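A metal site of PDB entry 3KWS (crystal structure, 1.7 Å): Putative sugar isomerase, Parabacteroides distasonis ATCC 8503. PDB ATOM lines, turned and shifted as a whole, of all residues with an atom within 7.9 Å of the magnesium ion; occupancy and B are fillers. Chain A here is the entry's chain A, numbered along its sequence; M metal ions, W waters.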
ATOM      1  N   GLN A  31      25.458 -16.949 -12.407  1.00  0.00           N
ATOM      2  CA  GLN A  31      25.254 -17.244 -11.005  1.00  0.00           C
ATOM      3  C   GLN A  31      24.301 -18.445 -10.918  1.00  0.00           C
ATOM      4  O   GLN A  31      23.537 -18.735 -11.833  1.00  0.00           O
ATOM      5  CB  GLN A  31      24.702 -16.048 -10.200  1.00  0.00           C
ATOM      6  CG  GLN A  31      25.813 -15.062  -9.880  1.00  0.00           C
ATOM      7  CD  GLN A  31      25.382 -13.954  -8.969  1.00  0.00           C
ATOM      8  OE1 GLN A  31      24.186 -13.756  -8.714  1.00  0.00           O
ATOM      9  NE2 GLN A  31      26.359 -13.218  -8.442  1.00  0.00           N
ATOM     10  N   GLU A  56      29.031 -19.479 -11.215  1.00  0.00           N
ATOM     11  CA  GLU A  56      29.379 -18.579 -10.110  1.00  0.00           C
ATOM     12  C   GLU A  56      28.512 -18.852  -8.885  1.00  0.00           C
ATOM     13  O   GLU A  56      27.433 -18.289  -8.779  1.00  0.00           O
ATOM     14  CB  GLU A  56      29.256 -17.104 -10.551  1.00  0.00           C
ATOM     15  CG  GLU A  56      29.551 -16.092  -9.440  1.00  0.00           C
ATOM     16  CD  GLU A  56      29.413 -14.642  -9.893  1.00  0.00           C
ATOM     17  OE1 GLU A  56      29.536 -14.379 -11.113  1.00  0.00           O
ATOM     18  OE2 GLU A  56      29.234 -13.789  -8.997  1.00  0.00           O
ATOM     19  N   CYS A  84      30.734 -15.523  -5.296  1.00  0.00           N
ATOM     20  CA  CYS A  84      30.106 -14.292  -4.912  1.00  0.00           C
ATOM     21  C   CYS A  84      29.935 -14.209  -3.396  1.00  0.00           C
ATOM     22  O   CYS A  84      29.084 -14.855  -2.838  1.00  0.00           O
ATOM     23  CB  CYS A  84      28.778 -14.138  -5.611  1.00  0.00           C
ATOM     24  SG  CYS A  84      28.197 -12.425  -5.526  1.00  0.00           S
ATOM     25  N   ILE A 122      34.524 -12.436  -4.526  1.00  0.00           N
ATOM     26  CA  ILE A 122      34.002 -11.055  -4.568  1.00  0.00           C
ATOM     27  C   ILE A 122      33.678 -10.546  -3.192  1.00  0.00           C
ATOM     28  O   ILE A 122      33.030 -11.259  -2.396  1.00  0.00           O
ATOM     29  CB  ILE A 122      32.760 -10.983  -5.435  1.00  0.00           C
ATOM     30  CG1 ILE A 122      33.078 -11.538  -6.834  1.00  0.00           C
ATOM     31  CG2 ILE A 122      32.191  -9.569  -5.503  1.00  0.00           C
ATOM     32  CD1 ILE A 122      31.807 -11.767  -7.677  1.00  0.00           C
ATOM     33  N   VAL A 124      32.640  -6.733  -1.064  1.00  0.00           N
ATOM     34  CA  VAL A 124      32.274  -5.321  -0.897  1.00  0.00           C
ATOM     35  C   VAL A 124      32.787  -4.877   0.471  1.00  0.00           C
ATOM     36  O   VAL A 124      32.444  -5.473   1.486  1.00  0.00           O
ATOM     37  CB  VAL A 124      30.725  -5.181  -0.976  1.00  0.00           C
ATOM     38  CG1 VAL A 124      30.227  -3.834  -0.473  1.00  0.00           C
ATOM     39  CG2 VAL A 124      30.222  -5.474  -2.416  1.00  0.00           C
ATOM     40  N   GLU A 165      34.347  -5.273  -5.306  1.00  0.00           N
ATOM     41  CA  GLU A 165      33.200  -4.914  -6.135  1.00  0.00           C
ATOM     42  C   GLU A 165      32.634  -3.570  -5.756  1.00  0.00           C
ATOM     43  O   GLU A 165      32.084  -3.417  -4.653  1.00  0.00           O
ATOM     44  CB  GLU A 165      32.067  -5.950  -6.096  1.00  0.00           C
ATOM     45  CG  GLU A 165      30.973  -5.645  -7.117  1.00  0.00           C
ATOM     46  CD  GLU A 165      29.766  -6.557  -7.026  1.00  0.00           C
ATOM     47  OE1 GLU A 165      29.444  -7.073  -5.919  1.00  0.00           O
ATOM     48  OE2 GLU A 165      29.101  -6.710  -8.067  1.00  0.00           O
ATOM     49  N   PRO A 166      32.712  -2.599  -6.690  1.00  0.00           N
ATOM     50  CA  PRO A 166      32.039  -1.311  -6.488  1.00  0.00           C
ATOM     51  C   PRO A 166      30.533  -1.485  -6.697  1.00  0.00           C
ATOM     52  O   PRO A 166      30.120  -2.098  -7.697  1.00  0.00           O
ATOM     53  CB  PRO A 166      32.609  -0.445  -7.621  1.00  0.00           C
ATOM     54  CG  PRO A 166      33.730  -1.233  -8.240  1.00  0.00           C
ATOM     55  CD  PRO A 166      33.367  -2.652  -7.992  1.00  0.00           C
ATOM     56  N   LEU A 167      29.729  -0.884  -5.809  1.00  0.00           N
ATOM     57  CA  LEU A 167      28.276  -0.885  -5.909  1.00  0.00           C
ATOM     58  C   LEU A 167      27.757   0.528  -6.085  1.00  0.00           C
ATOM     59  O   LEU A 167      28.470   1.508  -5.785  1.00  0.00           O
ATOM     60  CB  LEU A 167      27.663  -1.503  -4.646  1.00  0.00           C
ATOM     61  CG  LEU A 167      28.228  -2.779  -4.067  1.00  0.00           C
ATOM     62  CD1 LEU A 167      27.341  -3.135  -2.858  1.00  0.00           C
ATOM     63  CD2 LEU A 167      28.192  -3.874  -5.117  1.00  0.00           C
ATOM     64  N   GLU A 171      23.138   1.075  -2.533  1.00  0.00           N
ATOM     65  CA  GLU A 171      23.651  -0.030  -1.746  1.00  0.00           C
ATOM     66  C   GLU A 171      24.915   0.274  -0.968  1.00  0.00           C
ATOM     67  O   GLU A 171      25.137  -0.346   0.075  1.00  0.00           O
ATOM     68  CB  GLU A 171      23.916  -1.262  -2.593  1.00  0.00           C
ATOM     69  CG  GLU A 171      22.656  -1.743  -3.302  1.00  0.00           C
ATOM     70  CD  GLU A 171      22.780  -3.110  -3.922  1.00  0.00           C
ATOM     71  OE1 GLU A 171      23.312  -4.029  -3.278  1.00  0.00           O
ATOM     72  OE2 GLU A 171      22.290  -3.288  -5.052  1.00  0.00           O
ATOM     73  N   MET A 196      36.576  -5.652 -10.015  1.00  0.00           N
ATOM     74  CA  MET A 196      35.579  -5.962 -11.034  1.00  0.00           C
ATOM     75  C   MET A 196      34.675  -4.771 -11.287  1.00  0.00           C
ATOM     76  O   MET A 196      34.713  -3.786 -10.540  1.00  0.00           O
ATOM     77  CB  MET A 196      34.729  -7.131 -10.596  1.00  0.00           C
ATOM     78  CG  MET A 196      33.858  -6.928  -9.343  1.00  0.00           C
ATOM     79  SD  MET A 196      32.661  -8.445  -9.087  1.00  0.00           S
ATOM     80  CE  MET A 196      31.517  -8.058 -10.587  1.00  0.00           C
ATOM     81  N   GLY A 197      33.826  -4.930 -12.296  1.00  0.00           N
ATOM     82  CA  GLY A 197      32.757  -3.967 -12.586  1.00  0.00           C
ATOM     83  C   GLY A 197      31.472  -4.759 -12.752  1.00  0.00           C
ATOM     84  O   GLY A 197      31.488  -5.856 -13.296  1.00  0.00           O
ATOM     85  N   ASP A 198      30.359  -4.191 -12.288  1.00  0.00           N
ATOM     86  CA  ASP A 198      29.047  -4.814 -12.413  1.00  0.00           C
ATOM     87  C   ASP A 198      28.221  -3.844 -13.252  1.00  0.00           C
ATOM     88  O   ASP A 198      27.995  -2.707 -12.852  1.00  0.00           O
ATOM     89  CB  ASP A 198      28.471  -5.016 -11.019  1.00  0.00           C
ATOM     90  CG  ASP A 198      27.079  -5.607 -10.998  1.00  0.00           C
ATOM     91  OD1 ASP A 198      26.241  -5.224 -11.847  1.00  0.00           O
ATOM     92  OD2 ASP A 198      26.798  -6.410 -10.090  1.00  0.00           O
ATOM     93  N   PHE A 199      27.833  -4.265 -14.458  1.00  0.00           N
ATOM     94  CA  PHE A 199      27.079  -3.354 -15.332  1.00  0.00           C
ATOM     95  C   PHE A 199      25.835  -2.683 -14.693  1.00  0.00           C
ATOM     96  O   PHE A 199      25.517  -1.590 -15.054  1.00  0.00           O
ATOM     97  CB  PHE A 199      26.642  -4.082 -16.602  1.00  0.00           C
ATOM     98  CG  PHE A 199      27.679  -4.125 -17.707  1.00  0.00           C
ATOM     99  CD1 PHE A 199      27.947  -3.010 -18.496  1.00  0.00           C
ATOM    100  CD2 PHE A 199      28.312  -5.331 -18.039  1.00  0.00           C
ATOM    101  CE1 PHE A 199      28.824  -3.077 -19.573  1.00  0.00           C
ATOM    102  CE2 PHE A 199      29.203  -5.403 -19.133  1.00  0.00           C
ATOM    103  CZ  PHE A 199      29.446  -4.271 -19.900  1.00  0.00           C
ATOM    104  N   TRP A 200      25.141  -3.358 -13.791  1.00  0.00           N
ATOM    105  CA  TRP A 200      24.031  -2.767 -13.097  1.00  0.00           C
ATOM    106  C   TRP A 200      24.531  -1.517 -12.311  1.00  0.00           C
ATOM    107  O   TRP A 200      24.034  -0.395 -12.496  1.00  0.00           O
ATOM    108  CB  TRP A 200      23.348  -3.756 -12.170  1.00  0.00           C
ATOM    109  CG  TRP A 200      22.375  -3.093 -11.228  1.00  0.00           C
ATOM    110  CD1 TRP A 200      22.537  -2.923  -9.900  1.00  0.00           C
ATOM    111  CD2 TRP A 200      21.161  -2.436 -11.581  1.00  0.00           C
ATOM    112  NE1 TRP A 200      21.485  -2.253  -9.373  1.00  0.00           N
ATOM    113  CE2 TRP A 200      20.618  -1.918 -10.389  1.00  0.00           C
ATOM    114  CE3 TRP A 200      20.424  -2.297 -12.783  1.00  0.00           C
ATOM    115  CZ2 TRP A 200      19.392  -1.227 -10.345  1.00  0.00           C
ATOM    116  CZ3 TRP A 200      19.215  -1.582 -12.745  1.00  0.00           C
ATOM    117  CH2 TRP A 200      18.703  -1.079 -11.527  1.00  0.00           C
ATOM    118  N   HIS A 201      25.485  -1.732 -11.444  1.00  0.00           N
ATOM    119  CA  HIS A 201      26.017  -0.647 -10.617  1.00  0.00           C
ATOM    120  C   HIS A 201      26.642   0.449 -11.475  1.00  0.00           C
ATOM    121  O   HIS A 201      26.465   1.650 -11.166  1.00  0.00           O
ATOM    122  CB  HIS A 201      26.987  -1.207  -9.596  1.00  0.00           C
ATOM    123  CG  HIS A 201      26.328  -2.170  -8.662  1.00  0.00           C
ATOM    124  ND1 HIS A 201      25.245  -1.816  -7.897  1.00  0.00           N
ATOM    125  CD2 HIS A 201      26.601  -3.469  -8.351  1.00  0.00           C
ATOM    126  CE1 HIS A 201      24.849  -2.858  -7.192  1.00  0.00           C
ATOM    127  NE2 HIS A 201      25.659  -3.883  -7.445  1.00  0.00           N
ATOM    128  N   HIS A 222      36.751  -9.932 -13.053  1.00  0.00           N
ATOM    129  CA  HIS A 222      35.406 -10.441 -13.234  1.00  0.00           C
ATOM    130  C   HIS A 222      34.520  -9.297 -13.676  1.00  0.00           C
ATOM    131  O   HIS A 222      34.894  -8.129 -13.512  1.00  0.00           O
ATOM    132  CB  HIS A 222      34.898 -11.029 -11.914  1.00  0.00           C
ATOM    133  CG  HIS A 222      33.697 -11.898 -12.045  1.00  0.00           C
ATOM    134  ND1 HIS A 222      33.719 -13.092 -12.737  1.00  0.00           N
ATOM    135  CD2 HIS A 222      32.457 -11.798 -11.495  1.00  0.00           C
ATOM    136  CE1 HIS A 222      32.549 -13.693 -12.601  1.00  0.00           C
ATOM    137  NE2 HIS A 222      31.763 -12.927 -11.843  1.00  0.00           N
ATOM    138  N   VAL A 223      33.359  -9.660 -14.238  1.00  0.00           N
ATOM    139  CA  VAL A 223      32.330  -8.708 -14.653  1.00  0.00           C
ATOM    140  C   VAL A 223      30.957  -9.307 -14.348  1.00  0.00           C
ATOM    141  O   VAL A 223      30.742 -10.504 -14.589  1.00  0.00           O
ATOM    142  CB  VAL A 223      32.398  -8.350 -16.174  1.00  0.00           C
ATOM    143  CG1 VAL A 223      31.214  -7.445 -16.636  1.00  0.00           C
ATOM    144  CG2 VAL A 223      33.760  -7.662 -16.529  1.00  0.00           C
ATOM    145  N   HIS A 224      30.057  -8.478 -13.823  1.00  0.00           N
ATOM    146  CA  HIS A 224      28.654  -8.857 -13.669  1.00  0.00           C
ATOM    147  C   HIS A 224      27.785  -8.141 -14.735  1.00  0.00           C
ATOM    148  O   HIS A 224      28.027  -6.989 -15.110  1.00  0.00           O
ATOM    149  CB  HIS A 224      28.092  -8.559 -12.270  1.00  0.00           C
ATOM    150  CG  HIS A 224      28.448  -9.557 -11.233  1.00  0.00           C
ATOM    151  ND1 HIS A 224      28.409  -9.287  -9.871  1.00  0.00           N
ATOM    152  CD2 HIS A 224      28.854 -10.843 -11.343  1.00  0.00           C
ATOM    153  CE1 HIS A 224      28.739 -10.382  -9.215  1.00  0.00           C
ATOM    154  NE2 HIS A 224      29.032 -11.335 -10.074  1.00  0.00           N
ATOM    155  N   VAL A 225      26.739  -8.832 -15.209  1.00  0.00           N
ATOM    156  CA  VAL A 225      25.850  -8.247 -16.192  1.00  0.00           C
ATOM    157  C   VAL A 225      24.382  -8.463 -15.745  1.00  0.00           C
ATOM    158  O   VAL A 225      24.045  -9.465 -15.048  1.00  0.00           O
ATOM    159  CB  VAL A 225      26.147  -8.787 -17.656  1.00  0.00           C
ATOM    160  CG1 VAL A 225      25.819 -10.319 -17.773  1.00  0.00           C
ATOM    161  CG2 VAL A 225      25.424  -7.906 -18.714  1.00  0.00           C
ATOM    162  N   ARG A 231      17.398  -4.501 -13.404  1.00  0.00           N
ATOM    163  CA  ARG A 231      18.333  -5.519 -12.946  1.00  0.00           C
ATOM    164  C   ARG A 231      17.807  -6.942 -13.133  1.00  0.00           C
ATOM    165  O   ARG A 231      17.867  -7.822 -12.241  1.00  0.00           O
ATOM    166  CB  ARG A 231      18.708  -5.230 -11.500  1.00  0.00           C
ATOM    167  CG  ARG A 231      19.999  -5.935 -11.078  1.00  0.00           C
ATOM    168  CD  ARG A 231      20.328  -5.648  -9.630  1.00  0.00           C
ATOM    169  NE  ARG A 231      21.641  -6.128  -9.281  1.00  0.00           N
ATOM    170  CZ  ARG A 231      22.192  -5.935  -8.091  1.00  0.00           C
ATOM    171  NH1 ARG A 231      21.517  -5.335  -7.115  1.00  0.00           N
ATOM    172  NH2 ARG A 231      23.422  -6.371  -7.875  1.00  0.00           N
ATOM    173  N   SER A 260      29.553 -12.499 -16.131  1.00  0.00           N
ATOM    174  CA  SER A 260      28.640 -13.338 -15.386  1.00  0.00           C
ATOM    175  C   SER A 260      27.316 -12.686 -15.040  1.00  0.00           C
ATOM    176  O   SER A 260      27.244 -11.544 -14.568  1.00  0.00           O
ATOM    177  CB  SER A 260      29.325 -13.838 -14.120  1.00  0.00           C
ATOM    178  OG  SER A 260      28.662 -14.988 -13.575  1.00  0.00           O
ATOM    179  N   PHE A 261      26.233 -13.405 -15.301  1.00  0.00           N
ATOM    180  CA  PHE A 261      24.912 -12.913 -15.031  1.00  0.00           C
ATOM    181  C   PHE A 261      24.610 -12.863 -13.521  1.00  0.00           C
ATOM    182  O   PHE A 261      24.702 -13.882 -12.838  1.00  0.00           O
ATOM    183  CB  PHE A 261      23.838 -13.858 -15.616  1.00  0.00           C
ATOM    184  CG  PHE A 261      23.608 -13.775 -17.109  1.00  0.00           C
ATOM    185  CD1 PHE A 261      24.633 -13.864 -18.022  1.00  0.00           C
ATOM    186  CD2 PHE A 261      22.315 -13.764 -17.590  1.00  0.00           C
ATOM    187  CE1 PHE A 261      24.361 -13.864 -19.400  1.00  0.00           C
ATOM    188  CE2 PHE A 261      22.024 -13.775 -18.962  1.00  0.00           C
ATOM    189  CZ  PHE A 261      23.039 -13.800 -19.854  1.00  0.00           C
ATOM    190  N   GLU A 262      24.231 -11.673 -13.025  1.00  0.00           N
ATOM    191  CA  GLU A 262      23.749 -11.498 -11.665  1.00  0.00           C
ATOM    192  C   GLU A 262      22.540 -10.595 -11.834  1.00  0.00           C
ATOM    193  O   GLU A 262      22.664  -9.370 -11.944  1.00  0.00           O
ATOM    194  CB  GLU A 262      24.766 -10.842 -10.764  1.00  0.00           C
ATOM    195  CG  GLU A 262      24.197 -10.546  -9.394  1.00  0.00           C
ATOM    196  CD  GLU A 262      25.181  -9.840  -8.530  1.00  0.00           C
ATOM    197  OE1 GLU A 262      25.522  -8.674  -8.860  1.00  0.00           O
ATOM    198  OE2 GLU A 262      25.582 -10.427  -7.536  1.00  0.00           O
ATOM    199  N   CYS A 263      21.377 -11.199 -11.836  1.00  0.00           N
ATOM    200  CA  CYS A 263      20.183 -10.449 -12.132  1.00  0.00           C
ATOM    201  C   CYS A 263      18.951 -11.316 -11.848  1.00  0.00           C
ATOM    202  O   CYS A 263      19.028 -12.527 -11.647  1.00  0.00           O
ATOM    203  CB  CYS A 263      20.175 -10.040 -13.606  1.00  0.00           C
ATOM    204  SG  CYS A 263      20.240 -11.451 -14.771  1.00  0.00           S
HETATM  205 MG    MG M   1      27.451  -7.717  -8.627  1.00  0.00          MG
HETATM  206  O   HOH W   1      27.816  -9.015  -6.935  1.00  0.00           O
HETATM  207  O   HOH W   2      26.374  -6.625  -6.989  1.00  0.00           O
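The magnesium ion is bound by OE2 of Glu 165 (2.0 Å), OD2 of Asp 198 (2.1 Å), water W1 (2.2 Å), OE1 of Glu 262 (2.2 Å), ND1 of His 224 (2.2 Å) and water W2 (2.2 Å).
OE2 of Glu 262 is in hydrogen-bond range of NE2 of Gln 31, at 3.0 Å.
The guanidinium group (NH2) of Arg 231 sits close to the side-chain carboxylate (OE1) of Glu 262, at 3.3 Å.
The side-chain carboxylate of Asp 198 is in hydrogen-bond range of the backbone NH of Trp 200 (2.9 Å).
The backbone NH of Phe 199 is in hydrogen-bond range of the backbone carbonyl oxygen of His 224.
N of His 224 sits at hydrogen-bond distance from O of Gly 197, 3.0 Å away.
The backbone carbonyl oxygen of Val 225 is in hydrogen-bond range of the backbone NH of Glu 262, 3.0 Å away.
OE2 of Glu 56 is in hydrogen-bond range of NE2 of His 224.
Water W2 lies within hydrogen-bond range of a ring nitrogen (NE2) of His 201 (2.9 Å), the guanidinium group of Arg 231 (3.1 Å) and the side-chain carboxylate of Glu 165 (3.3 Å).
Water W1 lies within hydrogen-bond range of the side-chain carboxylate of Glu 262 (2.7 Å), the side-chain carboxylate of Glu 165 (2.7 Å) and the side-chain sulfur of Cys 84 (3.7 Å).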
